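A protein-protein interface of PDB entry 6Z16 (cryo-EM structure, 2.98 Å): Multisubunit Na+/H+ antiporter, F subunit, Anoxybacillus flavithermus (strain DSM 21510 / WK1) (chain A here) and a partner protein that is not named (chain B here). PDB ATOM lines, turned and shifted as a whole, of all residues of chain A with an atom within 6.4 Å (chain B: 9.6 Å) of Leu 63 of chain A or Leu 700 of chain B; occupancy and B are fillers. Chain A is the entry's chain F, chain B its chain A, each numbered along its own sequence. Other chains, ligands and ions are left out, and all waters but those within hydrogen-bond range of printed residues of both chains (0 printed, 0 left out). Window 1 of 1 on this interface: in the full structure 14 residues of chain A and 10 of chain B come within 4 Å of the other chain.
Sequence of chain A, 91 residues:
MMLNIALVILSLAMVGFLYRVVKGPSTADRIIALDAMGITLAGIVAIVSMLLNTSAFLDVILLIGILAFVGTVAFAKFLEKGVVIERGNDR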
ATOM      1  N   LEU A  58      22.083  -1.798  36.930  1.00  0.00           N
ATOM      2  CA  LEU A  58      21.618  -0.503  37.423  1.00  0.00           C
ATOM      3  C   LEU A  58      21.715   0.563  36.338  1.00  0.00           C
ATOM      4  O   LEU A  58      20.935   1.536  36.327  1.00  0.00           O
ATOM      5  CB  LEU A  58      22.424  -0.065  38.647  1.00  0.00           C
ATOM      6  CG  LEU A  58      22.339  -0.872  39.953  1.00  0.00           C
ATOM      7  CD1 LEU A  58      20.938  -1.341  40.286  1.00  0.00           C
ATOM      8  CD2 LEU A  58      23.317  -2.014  40.015  1.00  0.00           C
ATOM      9  N   ASP A  59      22.669   0.373  35.423  1.00  0.00           N
ATOM     10  CA  ASP A  59      22.783   1.215  34.242  1.00  0.00           C
ATOM     11  C   ASP A  59      21.537   1.126  33.384  1.00  0.00           C
ATOM     12  O   ASP A  59      21.145   2.114  32.757  1.00  0.00           O
ATOM     13  CB  ASP A  59      24.008   0.797  33.435  1.00  0.00           C
ATOM     14  CG  ASP A  59      25.307   1.068  34.162  1.00  0.00           C
ATOM     15  OD1 ASP A  59      25.367   2.049  34.936  1.00  0.00           O
ATOM     16  OD2 ASP A  59      26.267   0.295  33.964  1.00  0.00           O
ATOM     17  N   VAL A  60      20.893  -0.044  33.373  1.00  0.00           N
ATOM     18  CA  VAL A  60      19.617  -0.218  32.689  1.00  0.00           C
ATOM     19  C   VAL A  60      18.547   0.659  33.330  1.00  0.00           C
ATOM     20  O   VAL A  60      17.712   1.240  32.636  1.00  0.00           O
ATOM     21  CB  VAL A  60      19.223  -1.709  32.690  1.00  0.00           C
ATOM     22  CG1 VAL A  60      17.909  -1.941  31.985  1.00  0.00           C
ATOM     23  CG2 VAL A  60      20.324  -2.560  32.074  1.00  0.00           C
ATOM     24  N   ILE A  61      18.598   0.823  34.654  1.00  0.00           N
ATOM     25  CA  ILE A  61      17.588   1.609  35.364  1.00  0.00           C
ATOM     26  C   ILE A  61      17.724   3.089  35.036  1.00  0.00           C
ATOM     27  O   ILE A  61      16.742   3.761  34.676  1.00  0.00           O
ATOM     28  CB  ILE A  61      17.700   1.361  36.876  1.00  0.00           C
ATOM     29  CG1 ILE A  61      17.410  -0.100  37.182  1.00  0.00           C
ATOM     30  CG2 ILE A  61      16.778   2.290  37.646  1.00  0.00           C
ATOM     31  CD1 ILE A  61      17.820  -0.495  38.542  1.00  0.00           C
ATOM     32  N   LEU A  62      18.949   3.617  35.135  1.00  0.00           N
ATOM     33  CA  LEU A  62      19.144   5.022  34.779  1.00  0.00           C
ATOM     34  C   LEU A  62      18.947   5.259  33.284  1.00  0.00           C
ATOM     35  O   LEU A  62      18.480   6.337  32.880  1.00  0.00           O
ATOM     36  CB  LEU A  62      20.521   5.492  35.247  1.00  0.00           C
ATOM     37  CG  LEU A  62      20.894   6.956  35.022  1.00  0.00           C
ATOM     38  CD1 LEU A  62      19.833   7.869  35.581  1.00  0.00           C
ATOM     39  CD2 LEU A  62      22.214   7.245  35.692  1.00  0.00           C
ATOM     40  N   LEU A  63      19.201   4.233  32.464  1.00  0.00           N
ATOM     41  CA  LEU A  63      18.934   4.317  31.035  1.00  0.00           C
ATOM     42  C   LEU A  63      17.441   4.402  30.748  1.00  0.00           C
ATOM     43  O   LEU A  63      17.017   5.180  29.890  1.00  0.00           O
ATOM     44  CB  LEU A  63      19.536   3.110  30.330  1.00  0.00           C
ATOM     45  CG  LEU A  63      19.521   3.209  28.813  1.00  0.00           C
ATOM     46  CD1 LEU A  63      20.493   4.274  28.381  1.00  0.00           C
ATOM     47  CD2 LEU A  63      19.855   1.899  28.180  1.00  0.00           C
ATOM     48  N   ILE A  64      16.633   3.598  31.442  1.00  0.00           N
ATOM     49  CA  ILE A  64      15.183   3.640  31.260  1.00  0.00           C
ATOM     50  C   ILE A  64      14.632   4.995  31.684  1.00  0.00           C
ATOM     51  O   ILE A  64      13.756   5.559  31.011  1.00  0.00           O
ATOM     52  CB  ILE A  64      14.520   2.473  32.019  1.00  0.00           C
ATOM     53  CG1 ILE A  64      14.803   1.151  31.318  1.00  0.00           C
ATOM     54  CG2 ILE A  64      13.039   2.646  32.094  1.00  0.00           C
ATOM     55  CD1 ILE A  64      14.500  -0.035  32.169  1.00  0.00           C
ATOM     56  N   GLY A  65      15.194   5.573  32.752  1.00  0.00           N
ATOM     57  CA  GLY A  65      14.784   6.915  33.156  1.00  0.00           C
ATOM     58  C   GLY A  65      15.078   7.980  32.110  1.00  0.00           C
ATOM     59  O   GLY A  65      14.200   8.782  31.751  1.00  0.00           O
ATOM     60  N   ILE A  66      16.306   7.978  31.574  1.00  0.00           N
ATOM     61  CA  ILE A  66      16.663   9.018  30.608  1.00  0.00           C
ATOM     62  C   ILE A  66      15.931   8.811  29.277  1.00  0.00           C
ATOM     63  O   ILE A  66      15.488   9.787  28.655  1.00  0.00           O
ATOM     64  CB  ILE A  66      18.203   9.119  30.466  1.00  0.00           C
ATOM     65  CG1 ILE A  66      18.838   7.823  29.989  1.00  0.00           C
ATOM     66  CG2 ILE A  66      18.865   9.453  31.795  1.00  0.00           C
ATOM     67  CD1 ILE A  66      20.374   7.830  30.002  1.00  0.00           C
ATOM     68  N   LEU A  67      15.705   7.552  28.870  1.00  0.00           N
ATOM     69  CA  LEU A  67      14.944   7.263  27.654  1.00  0.00           C
ATOM     70  C   LEU A  67      13.483   7.669  27.781  1.00  0.00           C
ATOM     71  O   LEU A  67      12.906   8.208  26.827  1.00  0.00           O
ATOM     72  CB  LEU A  67      15.044   5.778  27.308  1.00  0.00           C
ATOM     73  CG  LEU A  67      16.072   5.294  26.287  1.00  0.00           C
ATOM     74  CD1 LEU A  67      17.475   5.599  26.695  1.00  0.00           C
ATOM     75  CD2 LEU A  67      15.919   3.810  26.129  1.00  0.00           C
ATOM     76  N   ALA A  68      12.873   7.425  28.948  1.00  0.00           N
ATOM     77  CA  ALA A  68      11.487   7.822  29.164  1.00  0.00           C
ATOM     78  C   ALA A  68      11.332   9.335  29.126  1.00  0.00           C
ATOM     79  O   ALA A  68      10.392   9.845  28.501  1.00  0.00           O
ATOM     80  CB  ALA A  68      10.980   7.261  30.491  1.00  0.00           C
ATOM     81  N   GLY B 683       9.751  -4.777  21.402  1.00  0.00           N
ATOM     82  CA  GLY B 683      11.160  -4.433  21.573  1.00  0.00           C
ATOM     83  C   GLY B 683      11.572  -4.273  23.028  1.00  0.00           C
ATOM     84  O   GLY B 683      12.599  -4.814  23.462  1.00  0.00           O
ATOM     85  N   TYR B 684      10.757  -3.560  23.811  1.00  0.00           N
ATOM     86  CA  TYR B 684      11.089  -3.367  25.223  1.00  0.00           C
ATOM     87  C   TYR B 684      10.957  -4.661  26.016  1.00  0.00           C
ATOM     88  O   TYR B 684      11.713  -4.890  26.965  1.00  0.00           O
ATOM     89  CB  TYR B 684      10.230  -2.265  25.847  1.00  0.00           C
ATOM     90  CG  TYR B 684      10.525  -0.886  25.298  1.00  0.00           C
ATOM     91  CD1 TYR B 684      11.728  -0.268  25.556  1.00  0.00           C
ATOM     92  CD2 TYR B 684       9.577  -0.179  24.579  1.00  0.00           C
ATOM     93  CE1 TYR B 684      12.006   0.984  25.068  1.00  0.00           C
ATOM     94  CE2 TYR B 684       9.844   1.074  24.079  1.00  0.00           C
ATOM     95  CZ  TYR B 684      11.057   1.653  24.336  1.00  0.00           C
ATOM     96  OH  TYR B 684      11.327   2.907  23.854  1.00  0.00           O
ATOM     97  N   VAL B 686      11.591  -7.688  24.652  1.00  0.00           N
ATOM     98  CA  VAL B 686      12.792  -8.441  24.289  1.00  0.00           C
ATOM     99  C   VAL B 686      13.980  -7.955  25.111  1.00  0.00           C
ATOM    100  O   VAL B 686      14.814  -8.753  25.561  1.00  0.00           O
ATOM    101  CB  VAL B 686      13.047  -8.350  22.768  1.00  0.00           C
ATOM    102  CG1 VAL B 686      14.429  -8.846  22.394  1.00  0.00           C
ATOM    103  CG2 VAL B 686      12.041  -9.194  22.020  1.00  0.00           C
ATOM    104  N   ALA B 687      14.037  -6.644  25.373  1.00  0.00           N
ATOM    105  CA  ALA B 687      15.031  -6.109  26.303  1.00  0.00           C
ATOM    106  C   ALA B 687      14.844  -6.659  27.714  1.00  0.00           C
ATOM    107  O   ALA B 687      15.823  -6.924  28.421  1.00  0.00           O
ATOM    108  CB  ALA B 687      14.968  -4.586  26.316  1.00  0.00           C
ATOM    109  N   LEU B 688      13.595  -6.854  28.138  1.00  0.00           N
ATOM    110  CA  LEU B 688      13.367  -7.432  29.461  1.00  0.00           C
ATOM    111  C   LEU B 688      13.727  -8.917  29.503  1.00  0.00           C
ATOM    112  O   LEU B 688      14.160  -9.416  30.550  1.00  0.00           O
ATOM    113  CB  LEU B 688      11.921  -7.194  29.894  1.00  0.00           C
ATOM    114  CG  LEU B 688      11.534  -7.583  31.320  1.00  0.00           C
ATOM    115  CD1 LEU B 688      12.397  -6.846  32.326  1.00  0.00           C
ATOM    116  CD2 LEU B 688      10.073  -7.271  31.559  1.00  0.00           C
ATOM    117  N   PHE B 690      16.301  -9.980  27.761  1.00  0.00           N
ATOM    118  CA  PHE B 690      17.756  -9.858  27.828  1.00  0.00           C
ATOM    119  C   PHE B 690      18.227  -9.593  29.252  1.00  0.00           C
ATOM    120  O   PHE B 690      19.270 -10.107  29.669  1.00  0.00           O
ATOM    121  CB  PHE B 690      18.225  -8.747  26.894  1.00  0.00           C
ATOM    122  CG  PHE B 690      18.182  -9.111  25.439  1.00  0.00           C
ATOM    123  CD1 PHE B 690      18.202 -10.436  25.036  1.00  0.00           C
ATOM    124  CD2 PHE B 690      18.107  -8.121  24.473  1.00  0.00           C
ATOM    125  CE1 PHE B 690      18.162 -10.765  23.699  1.00  0.00           C
ATOM    126  CE2 PHE B 690      18.063  -8.444  23.138  1.00  0.00           C
ATOM    127  CZ  PHE B 690      18.090  -9.765  22.750  1.00  0.00           C
ATOM    128  N   VAL B 691      17.470  -8.785  30.003  1.00  0.00           N
ATOM    129  CA  VAL B 691      17.715  -8.628  31.439  1.00  0.00           C
ATOM    130  C   VAL B 691      17.551  -9.962  32.150  1.00  0.00           C
ATOM    131  O   VAL B 691      18.400 -10.380  32.944  1.00  0.00           O
ATOM    132  CB  VAL B 691      16.769  -7.571  32.037  1.00  0.00           C
ATOM    133  CG1 VAL B 691      16.899  -7.535  33.541  1.00  0.00           C
ATOM    134  CG2 VAL B 691      17.050  -6.203  31.469  1.00  0.00           C
ATOM    135  N   ALA B 695      21.911 -10.816  30.297  1.00  0.00           N
ATOM    136  CA  ALA B 695      22.623 -10.151  29.206  1.00  0.00           C
ATOM    137  C   ALA B 695      22.496  -8.640  29.349  1.00  0.00           C
ATOM    138  O   ALA B 695      21.568  -8.033  28.799  1.00  0.00           O
ATOM    139  CB  ALA B 695      22.094 -10.606  27.851  1.00  0.00           C
ATOM    140  N   PRO B 696      23.415  -7.995  30.075  1.00  0.00           N
ATOM    141  CA  PRO B 696      23.240  -6.557  30.359  1.00  0.00           C
ATOM    142  C   PRO B 696      23.488  -5.646  29.167  1.00  0.00           C
ATOM    143  O   PRO B 696      22.728  -4.680  28.961  1.00  0.00           O
ATOM    144  CB  PRO B 696      24.261  -6.306  31.476  1.00  0.00           C
ATOM    145  CG  PRO B 696      24.535  -7.655  32.067  1.00  0.00           C
ATOM    146  CD  PRO B 696      24.451  -8.602  30.926  1.00  0.00           C
ATOM    147  N   ASP B 697      24.546  -5.920  28.391  1.00  0.00           N
ATOM    148  CA  ASP B 697      24.904  -5.087  27.242  1.00  0.00           C
ATOM    149  C   ASP B 697      23.810  -5.110  26.185  1.00  0.00           C
ATOM    150  O   ASP B 697      23.474  -4.072  25.588  1.00  0.00           O
ATOM    151  CB  ASP B 697      26.219  -5.583  26.643  1.00  0.00           C
ATOM    152  CG  ASP B 697      27.410  -5.320  27.541  1.00  0.00           C
ATOM    153  OD1 ASP B 697      27.397  -4.304  28.259  1.00  0.00           O
ATOM    154  OD2 ASP B 697      28.359  -6.131  27.533  1.00  0.00           O
ATOM    155  N   LEU B 698      23.243  -6.296  25.964  1.00  0.00           N
ATOM    156  CA  LEU B 698      22.150  -6.478  25.020  1.00  0.00           C
ATOM    157  C   LEU B 698      20.927  -5.693  25.449  1.00  0.00           C
ATOM    158  O   LEU B 698      20.249  -5.091  24.614  1.00  0.00           O
ATOM    159  CB  LEU B 698      21.815  -7.963  24.902  1.00  0.00           C
ATOM    160  CG  LEU B 698      22.559  -8.868  23.926  1.00  0.00           C
ATOM    161  CD1 LEU B 698      24.011  -8.976  24.263  1.00  0.00           C
ATOM    162  CD2 LEU B 698      21.939 -10.241  24.007  1.00  0.00           C
ATOM    163  N   ALA B 699      20.664  -5.652  26.755  1.00  0.00           N
ATOM    164  CA  ALA B 699      19.523  -4.914  27.274  1.00  0.00           C
ATOM    165  C   ALA B 699      19.688  -3.412  27.078  1.00  0.00           C
ATOM    166  O   ALA B 699      18.751  -2.740  26.628  1.00  0.00           O
ATOM    167  CB  ALA B 699      19.332  -5.249  28.747  1.00  0.00           C
ATOM    168  N   LEU B 700      20.883  -2.883  27.378  1.00  0.00           N
ATOM    169  CA  LEU B 700      21.156  -1.451  27.205  1.00  0.00           C
ATOM    170  C   LEU B 700      21.003  -1.020  25.747  1.00  0.00           C
ATOM    171  O   LEU B 700      20.235  -0.089  25.423  1.00  0.00           O
ATOM    172  CB  LEU B 700      22.572  -1.147  27.694  1.00  0.00           C
ATOM    173  CG  LEU B 700      22.916  -1.313  29.175  1.00  0.00           C
ATOM    174  CD1 LEU B 700      24.415  -1.331  29.365  1.00  0.00           C
ATOM    175  CD2 LEU B 700      22.326  -0.183  29.975  1.00  0.00           C
ATOM    176  N   THR B 701      21.704  -1.723  24.850  1.00  0.00           N
ATOM    177  CA  THR B 701      21.663  -1.389  23.433  1.00  0.00           C
ATOM    178  C   THR B 701      20.286  -1.626  22.834  1.00  0.00           C
ATOM    179  O   THR B 701      19.844  -0.844  21.986  1.00  0.00           O
ATOM    180  CB  THR B 701      22.716  -2.198  22.692  1.00  0.00           C
ATOM    181  OG1 THR B 701      22.485  -3.590  22.930  1.00  0.00           O
ATOM    182  CG2 THR B 701      24.098  -1.838  23.193  1.00  0.00           C
ATOM    183  N   GLN B 702      19.576  -2.653  23.308  1.00  0.00           N
ATOM    184  CA  GLN B 702      18.244  -2.961  22.812  1.00  0.00           C
ATOM    185  C   GLN B 702      17.250  -1.870  23.173  1.00  0.00           C
ATOM    186  O   GLN B 702      16.443  -1.469  22.330  1.00  0.00           O
ATOM    187  CB  GLN B 702      17.793  -4.307  23.376  1.00  0.00           C
ATOM    188  CG  GLN B 702      16.471  -4.810  22.839  1.00  0.00           C
ATOM    189  CD  GLN B 702      16.576  -5.303  21.420  1.00  0.00           C
ATOM    190  OE1 GLN B 702      17.520  -5.998  21.068  1.00  0.00           O
ATOM    191  NE2 GLN B 702      15.608  -4.948  20.594  1.00  0.00           N
ATOM    192  N   LEU B 703      17.310  -1.363  24.413  1.00  0.00           N
ATOM    193  CA  LEU B 703      16.407  -0.296  24.837  1.00  0.00           C
ATOM    194  C   LEU B 703      16.618   0.973  24.021  1.00  0.00           C
ATOM    195  O   LEU B 703      15.651   1.564  23.511  1.00  0.00           O
ATOM    196  CB  LEU B 703      16.598  -0.007  26.324  1.00  0.00           C
ATOM    197  CG  LEU B 703      16.101  -1.035  27.336  1.00  0.00           C
ATOM    198  CD1 LEU B 703      16.685  -0.735  28.683  1.00  0.00           C
ATOM    199  CD2 LEU B 703      14.616  -1.011  27.435  1.00  0.00           C
ATOM    200  N   VAL B 704      17.883   1.376  23.841  1.00  0.00           N
ATOM    201  CA  VAL B 704      18.137   2.623  23.113  1.00  0.00           C
ATOM    202  C   VAL B 704      17.785   2.485  21.634  1.00  0.00           C
ATOM    203  O   VAL B 704      17.137   3.371  21.049  1.00  0.00           O
ATOM    204  CB  VAL B 704      19.592   3.071  23.315  1.00  0.00           C
ATOM    205  CG1 VAL B 704      19.895   4.296  22.479  1.00  0.00           C
ATOM    206  CG2 VAL B 704      19.802   3.388  24.752  1.00  0.00           C
ATOM    207  N   ILE B 705      18.154   1.357  21.020  1.00  0.00           N
ATOM    208  CA  ILE B 705      17.900   1.156  19.599  1.00  0.00           C
ATOM    209  C   ILE B 705      16.408   1.009  19.311  1.00  0.00           C
ATOM    210  O   ILE B 705      15.918   1.540  18.304  1.00  0.00           O
ATOM    211  CB  ILE B 705      18.747  -0.036  19.114  1.00  0.00           C
ATOM    212  CG1 ILE B 705      20.207   0.403  19.001  1.00  0.00           C
ATOM    213  CG2 ILE B 705      18.251  -0.611  17.805  1.00  0.00           C
ATOM    214  CD1 ILE B 705      21.172  -0.712  18.830  1.00  0.00           C
ATOM    215  N   GLU B 706      15.644   0.379  20.213  1.00  0.00           N
ATOM    216  CA  GLU B 706      14.203   0.318  20.000  1.00  0.00           C
ATOM    217  C   GLU B 706      13.533   1.667  20.179  1.00  0.00           C
ATOM    218  O   GLU B 706      12.577   1.960  19.459  1.00  0.00           O
ATOM    219  CB  GLU B 706      13.549  -0.713  20.911  1.00  0.00           C
ATOM    220  CG  GLU B 706      13.876  -2.115  20.488  1.00  0.00           C
ATOM    221  CD  GLU B 706      13.353  -2.447  19.104  1.00  0.00           C
ATOM    222  OE1 GLU B 706      12.221  -2.036  18.770  1.00  0.00           O
ATOM    223  OE2 GLU B 706      14.098  -3.085  18.331  1.00  0.00           O
ATOM    224  N   THR B 707      14.033   2.516  21.085  1.00  0.00           N
ATOM    225  CA  THR B 707      13.445   3.851  21.198  1.00  0.00           C
ATOM    226  C   THR B 707      13.696   4.681  19.940  1.00  0.00           C
ATOM    227  O   THR B 707      12.774   5.337  19.426  1.00  0.00           O
ATOM    228  CB  THR B 707      13.991   4.559  22.432  1.00  0.00           C
ATOM    229  OG1 THR B 707      13.795   3.719  23.571  1.00  0.00           O
ATOM    230  CG2 THR B 707      13.238   5.855  22.667  1.00  0.00           C
ATOM    231  N   ILE B 708      14.914   4.598  19.387  1.00  0.00           N
ATOM    232  CA  ILE B 708      15.232   5.342  18.166  1.00  0.00           C
ATOM    233  C   ILE B 708      14.433   4.808  16.977  1.00  0.00           C
ATOM    234  O   ILE B 708      13.903   5.580  16.163  1.00  0.00           O
ATOM    235  CB  ILE B 708      16.748   5.299  17.890  1.00  0.00           C
ATOM    236  CG1 ILE B 708      17.527   5.892  19.057  1.00  0.00           C
ATOM    237  CG2 ILE B 708      17.090   6.104  16.652  1.00  0.00           C
ATOM    238  CD1 ILE B 708      19.006   5.582  19.009  1.00  0.00           C
ATOM    239  N   ASN B 779      34.898  -7.642  31.801  1.00  0.00           N
ATOM    240  CA  ASN B 779      33.757  -7.862  30.928  1.00  0.00           C
ATOM    241  C   ASN B 779      34.143  -8.860  29.849  1.00  0.00           C
ATOM    242  O   ASN B 779      35.289  -8.906  29.410  1.00  0.00           O
ATOM    243  CB  ASN B 779      33.334  -6.544  30.288  1.00  0.00           C
ATOM    244  CG  ASN B 779      31.971  -6.606  29.662  1.00  0.00           C
ATOM    245  OD1 ASN B 779      31.308  -7.636  29.686  1.00  0.00           O
ATOM    246  ND2 ASN B 779      31.529  -5.490  29.112  1.00  0.00           N
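The side-chain hydroxyl of Thr 707 of chain B lies within hydrogen-bond range of the backbone carbonyl oxygen of Leu 703 of chain B, 2.8 Å away. OH of Tyr 684 of chain B is in hydrogen-bond range of OG1 of Thr 707 of chain B (2.6 Å).
Of the printed residues of chain B, Asp 59 of chain A touches Leu 700. Val 60 of chain A touches just these residues of chain B: Leu 700 and Leu 703. Of chain B, only Leu 700 and Val 704 come within 4 Å of Leu 63 of chain A. Ile 64 of chain A touches one residue of chain B. Gly 65 of chain A touches none of the printed residues of chain B. Ile 66 of chain A touches none of the printed residues of chain B. Of the printed residues of chain B, Leu 67 of chain A touches Leu 703 (3.5 Å), Val 704 (3.8 Å) and Thr 707 (3.3 Å). Printed residues of chain A within 4 Å of Leu 700 of chain B: Asp 59 (3.7 Å), Val 60 (3.7 Å) and Leu 63 (3.4 Å). Printed residues of chain A within 4 Å of Leu 703 of chain B: Val 60, Ile 64 and Leu 67. Of the printed residues of chain A, Thr 707 of chain B touches Leu 67. The nearest printed residue of chain B that does not touch Leu 67 of chain A is Tyr 684 of chain B (4.9 Å).
Printed residues of chain B that touch a printed residue of chain A: Leu 700, Leu 703, Val 704 and Thr 707. Hydrophobic or aromatic side chains of chain B within 4 Å of the printed part of chain A: Leu 700, Leu 703 and Val 704. Of the 11 printed residues of chain A, 5 touch a printed residue of chain B. Among the printed residues, 9 pairs touch across the chains.
Among the printed residues, merely in contact across the chains: Leu 67 of chain A with Thr 707 of chain B, Leu 63 of chain A with Leu 700 of chain B, Leu 67 of chain A with Leu 703 of chain B, Val 60 of chain A with Leu 700 of chain B, Val 60 of chain A with Leu 703 of chain B, Asp 59 of chain A with Leu 700 of chain B, Leu 63 of chain A with Val 704 of chain B, Ile 64 of chain A with Leu 703 of chain B and Leu 67 of chain A with Val 704 of chain B.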
